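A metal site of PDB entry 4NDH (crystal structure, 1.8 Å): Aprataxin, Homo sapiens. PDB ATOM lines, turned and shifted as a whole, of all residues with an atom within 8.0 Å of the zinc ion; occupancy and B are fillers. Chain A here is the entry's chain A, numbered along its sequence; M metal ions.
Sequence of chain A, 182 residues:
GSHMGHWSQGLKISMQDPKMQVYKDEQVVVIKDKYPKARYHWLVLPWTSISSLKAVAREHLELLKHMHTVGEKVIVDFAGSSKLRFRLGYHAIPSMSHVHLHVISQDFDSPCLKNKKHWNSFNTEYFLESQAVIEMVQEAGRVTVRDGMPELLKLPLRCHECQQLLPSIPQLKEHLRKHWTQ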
ATOM      1  N   ARG A 158     -21.620  21.902 -29.784  1.00  0.00           N
ATOM      2  CA  ARG A 158     -22.909  21.493 -29.245  1.00  0.00           C
ATOM      3  C   ARG A 158     -23.324  22.363 -28.073  1.00  0.00           C
ATOM      4  O   ARG A 158     -22.528  22.677 -27.193  1.00  0.00           O
ATOM      5  CB  ARG A 158     -22.901  20.015 -28.837  1.00  0.00           C
ATOM      6  CG  ARG A 158     -22.931  19.053 -30.010  1.00  0.00           C
ATOM      7  CD  ARG A 158     -23.240  17.637 -29.557  1.00  0.00           C
ATOM      8  NE  ARG A 158     -23.234  16.688 -30.669  1.00  0.00           N
ATOM      9  CZ  ARG A 158     -24.275  16.435 -31.442  1.00  0.00           C
ATOM     10  NH1 ARG A 158     -25.427  17.063 -31.244  1.00  0.00           N
ATOM     11  NH2 ARG A 158     -24.171  15.560 -32.434  1.00  0.00           N
ATOM     12  N   CYS A 159     -24.598  22.767 -28.080  1.00  0.00           N
ATOM     13  CA  CYS A 159     -25.130  23.593 -27.005  1.00  0.00           C
ATOM     14  C   CYS A 159     -25.030  22.844 -25.683  1.00  0.00           C
ATOM     15  O   CYS A 159     -25.259  21.631 -25.620  1.00  0.00           O
ATOM     16  CB  CYS A 159     -26.584  23.974 -27.285  1.00  0.00           C
ATOM     17  SG  CYS A 159     -27.295  25.025 -25.996  1.00  0.00           S
ATOM     18  N   HIS A 160     -24.667  23.549 -24.626  1.00  0.00           N
ATOM     19  CA  HIS A 160     -24.479  22.928 -23.323  1.00  0.00           C
ATOM     20  C   HIS A 160     -25.809  22.800 -22.588  1.00  0.00           C
ATOM     21  O   HIS A 160     -25.921  22.083 -21.602  1.00  0.00           O
ATOM     22  CB  HIS A 160     -23.511  23.748 -22.472  1.00  0.00           C
ATOM     23  CG  HIS A 160     -24.013  25.107 -22.125  1.00  0.00           C
ATOM     24  ND1 HIS A 160     -24.516  25.973 -23.078  1.00  0.00           N
ATOM     25  CD2 HIS A 160     -24.102  25.764 -20.941  1.00  0.00           C
ATOM     26  CE1 HIS A 160     -24.882  27.104 -22.490  1.00  0.00           C
ATOM     27  NE2 HIS A 160     -24.640  26.995 -21.188  1.00  0.00           N
ATOM     28  N   GLU A 161     -26.822  23.514 -23.075  1.00  0.00           N
ATOM     29  CA  GLU A 161     -28.128  23.492 -22.426  1.00  0.00           C
ATOM     30  C   GLU A 161     -29.076  22.453 -23.026  1.00  0.00           C
ATOM     31  O   GLU A 161     -29.755  21.725 -22.296  1.00  0.00           O
ATOM     32  CB  GLU A 161     -28.763  24.876 -22.430  1.00  0.00           C
ATOM     33  CG  GLU A 161     -27.957  25.947 -21.680  1.00  0.00           C
ATOM     34  CD  GLU A 161     -27.954  25.771 -20.168  1.00  0.00           C
ATOM     35  OE1 GLU A 161     -28.562  24.808 -19.661  1.00  0.00           O
ATOM     36  OE2 GLU A 161     -27.345  26.617 -19.471  1.00  0.00           O
ATOM     37  N   CYS A 162     -29.132  22.369 -24.354  1.00  0.00           N
ATOM     38  CA  CYS A 162     -30.075  21.465 -25.018  1.00  0.00           C
ATOM     39  C   CYS A 162     -29.391  20.476 -25.950  1.00  0.00           C
ATOM     40  O   CYS A 162     -30.058  19.692 -26.628  1.00  0.00           O
ATOM     41  CB  CYS A 162     -31.116  22.269 -25.799  1.00  0.00           C
ATOM     42  SG  CYS A 162     -30.456  23.056 -27.288  1.00  0.00           S
ATOM     43  N   GLN A 163     -28.057  20.527 -26.016  1.00  0.00           N
ATOM     44  CA  GLN A 163     -27.258  19.586 -26.796  1.00  0.00           C
ATOM     45  C   GLN A 163     -27.425  19.660 -28.317  1.00  0.00           C
ATOM     46  O   GLN A 163     -27.002  18.768 -29.040  1.00  0.00           O
ATOM     47  CB  GLN A 163     -27.433  18.143 -26.302  1.00  0.00           C
ATOM     48  CG  GLN A 163     -26.801  17.855 -24.948  1.00  0.00           C
ATOM     49  CD  GLN A 163     -27.607  18.423 -23.789  1.00  0.00           C
ATOM     50  OE1 GLN A 163     -28.811  18.164 -23.676  1.00  0.00           O
ATOM     51  NE2 GLN A 163     -26.965  19.195 -22.925  1.00  0.00           N
ATOM     52  N   GLN A 164     -28.030  20.737 -28.812  1.00  0.00           N
ATOM     53  CA  GLN A 164     -28.189  20.896 -30.265  1.00  0.00           C
ATOM     54  C   GLN A 164     -26.849  21.124 -30.958  1.00  0.00           C
ATOM     55  O   GLN A 164     -25.997  21.852 -30.460  1.00  0.00           O
ATOM     56  CB  GLN A 164     -29.142  22.051 -30.572  1.00  0.00           C
ATOM     57  CG  GLN A 164     -29.297  22.332 -32.062  1.00  0.00           C
ATOM     58  CD  GLN A 164     -30.376  23.343 -32.364  1.00  0.00           C
ATOM     59  OE1 GLN A 164     -31.347  23.492 -31.608  1.00  0.00           O
ATOM     60  NE2 GLN A 164     -30.225  24.060 -33.476  1.00  0.00           N
ATOM     61  N   LEU A 165     -26.668  20.489 -32.107  1.00  0.00           N
ATOM     62  CA  LEU A 165     -25.457  20.662 -32.907  1.00  0.00           C
ATOM     63  C   LEU A 165     -25.549  21.935 -33.750  1.00  0.00           C
ATOM     64  O   LEU A 165     -26.542  22.151 -34.444  1.00  0.00           O
ATOM     65  CB  LEU A 165     -25.239  19.454 -33.818  1.00  0.00           C
ATOM     66  CG  LEU A 165     -24.140  19.594 -34.879  1.00  0.00           C
ATOM     67  CD1 LEU A 165     -22.765  19.644 -34.230  1.00  0.00           C
ATOM     68  CD2 LEU A 165     -24.215  18.467 -35.894  1.00  0.00           C
ATOM     69  N   LEU A 166     -24.510  22.767 -33.675  1.00  0.00           N
ATOM     70  CA  LEU A 166     -24.430  24.001 -34.462  1.00  0.00           C
ATOM     71  C   LEU A 166     -23.187  23.976 -35.339  1.00  0.00           C
ATOM     72  O   LEU A 166     -22.126  23.516 -34.919  1.00  0.00           O
ATOM     73  CB  LEU A 166     -24.387  25.226 -33.537  1.00  0.00           C
ATOM     74  CG  LEU A 166     -25.712  25.739 -32.971  1.00  0.00           C
ATOM     75  CD1 LEU A 166     -26.730  25.956 -34.075  1.00  0.00           C
ATOM     76  CD2 LEU A 166     -26.266  24.803 -31.896  1.00  0.00           C
ATOM     77  N   LEU A 172     -23.677  29.263 -33.165  1.00  0.00           N
ATOM     78  CA  LEU A 172     -23.747  28.854 -31.757  1.00  0.00           C
ATOM     79  C   LEU A 172     -24.066  30.038 -30.871  1.00  0.00           C
ATOM     80  O   LEU A 172     -24.923  29.955 -29.980  1.00  0.00           O
ATOM     81  CB  LEU A 172     -22.435  28.204 -31.324  1.00  0.00           C
ATOM     82  CG  LEU A 172     -22.373  27.784 -29.848  1.00  0.00           C
ATOM     83  CD1 LEU A 172     -23.428  26.725 -29.553  1.00  0.00           C
ATOM     84  CD2 LEU A 172     -20.987  27.272 -29.493  1.00  0.00           C
ATOM     85  N   HIS A 175     -27.637  30.939 -31.170  1.00  0.00           N
ATOM     86  CA  HIS A 175     -28.474  29.934 -30.500  1.00  0.00           C
ATOM     87  C   HIS A 175     -28.506  30.124 -28.980  1.00  0.00           C
ATOM     88  O   HIS A 175     -29.557  30.015 -28.365  1.00  0.00           O
ATOM     89  CB  HIS A 175     -28.016  28.517 -30.843  1.00  0.00           C
ATOM     90  CG  HIS A 175     -28.737  27.449 -30.064  1.00  0.00           C
ATOM     91  ND1 HIS A 175     -29.881  26.831 -30.522  1.00  0.00           N
ATOM     92  CD2 HIS A 175     -28.480  26.909 -28.847  1.00  0.00           C
ATOM     93  CE1 HIS A 175     -30.297  25.953 -29.625  1.00  0.00           C
ATOM     94  NE2 HIS A 175     -29.466  25.980 -28.597  1.00  0.00           N
ATOM     95  N   LEU A 176     -27.351  30.423 -28.397  1.00  0.00           N
ATOM     96  CA  LEU A 176     -27.234  30.549 -26.938  1.00  0.00           C
ATOM     97  C   LEU A 176     -28.159  31.612 -26.337  1.00  0.00           C
ATOM     98  O   LEU A 176     -28.551  31.512 -25.169  1.00  0.00           O
ATOM     99  CB  LEU A 176     -25.789  30.842 -26.534  1.00  0.00           C
ATOM    100  CG  LEU A 176     -24.777  29.712 -26.721  1.00  0.00           C
ATOM    101  CD1 LEU A 176     -23.366  30.221 -26.487  1.00  0.00           C
ATOM    102  CD2 LEU A 176     -25.094  28.553 -25.780  1.00  0.00           C
ATOM    103  N   ARG A 177     -28.493  32.623 -27.134  1.00  0.00           N
ATOM    104  CA  ARG A 177     -29.403  33.673 -26.701  1.00  0.00           C
ATOM    105  C   ARG A 177     -30.767  33.115 -26.301  1.00  0.00           C
ATOM    106  O   ARG A 177     -31.450  33.665 -25.440  1.00  0.00           O
ATOM    107  CB  ARG A 177     -29.587  34.707 -27.807  1.00  0.00           C
ATOM    108  CG  ARG A 177     -28.389  35.592 -28.052  1.00  0.00           C
ATOM    109  CD  ARG A 177     -28.706  36.643 -29.106  1.00  0.00           C
ATOM    110  NE  ARG A 177     -28.152  37.950 -28.782  1.00  0.00           N
ATOM    111  CZ  ARG A 177     -28.853  38.974 -28.316  1.00  0.00           C
ATOM    112  NH1 ARG A 177     -30.163  38.853 -28.120  1.00  0.00           N
ATOM    113  NH2 ARG A 177     -28.253  40.127 -28.046  1.00  0.00           N
ATOM    114  N   LYS A 178     -31.152  32.005 -26.928  1.00  0.00           N
ATOM    115  CA  LYS A 178     -32.437  31.376 -26.642  1.00  0.00           C
ATOM    116  C   LYS A 178     -32.524  30.852 -25.209  1.00  0.00           C
ATOM    117  O   LYS A 178     -33.621  30.650 -24.687  1.00  0.00           O
ATOM    118  CB  LYS A 178     -32.717  30.245 -27.630  1.00  0.00           C
ATOM    119  CG  LYS A 178     -32.886  30.724 -29.065  1.00  0.00           C
ATOM    120  CD  LYS A 178     -33.255  29.575 -29.991  1.00  0.00           C
ATOM    121  CE  LYS A 178     -33.533  30.079 -31.398  1.00  0.00           C
ATOM    122  NZ  LYS A 178     -33.957  28.985 -32.313  1.00  0.00           N
ATOM    123  N   HIS A 179     -31.375  30.633 -24.585  1.00  0.00           N
ATOM    124  CA  HIS A 179     -31.340  30.052 -23.244  1.00  0.00           C
ATOM    125  C   HIS A 179     -31.138  31.078 -22.124  1.00  0.00           C
ATOM    126  O   HIS A 179     -30.746  30.721 -21.014  1.00  0.00           O
ATOM    127  CB  HIS A 179     -30.268  28.970 -23.150  1.00  0.00           C
ATOM    128  CG  HIS A 179     -30.536  27.789 -24.017  1.00  0.00           C
ATOM    129  ND1 HIS A 179     -31.606  26.943 -23.836  1.00  0.00           N
ATOM    130  CD2 HIS A 179     -29.858  27.305 -25.096  1.00  0.00           C
ATOM    131  CE1 HIS A 179     -31.587  26.000 -24.748  1.00  0.00           C
ATOM    132  NE2 HIS A 179     -30.536  26.197 -25.528  1.00  0.00           N
HETATM  133 ZN    ZN M   1     -29.488  25.049 -26.807  1.00  0.00          ZN
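SG of Cys 162 lies close to N of Gln 164.
N of Glu 161 lies close to SG of Cys 159 (3.3 Å).
The backbone NH (N) of Cys 159 is in hydrogen-bond range of the backbone carbonyl oxygen (O) of Gln 164 (2.9 Å).
The zinc ion is bound by NE2 of His 179 (2.0 Å), NE2 of His 175 (2.0 Å), SG of Cys 162 (2.3 Å) and SG of Cys 159 (2.3 Å).
The zinc ion has four donor atoms within binding distance.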
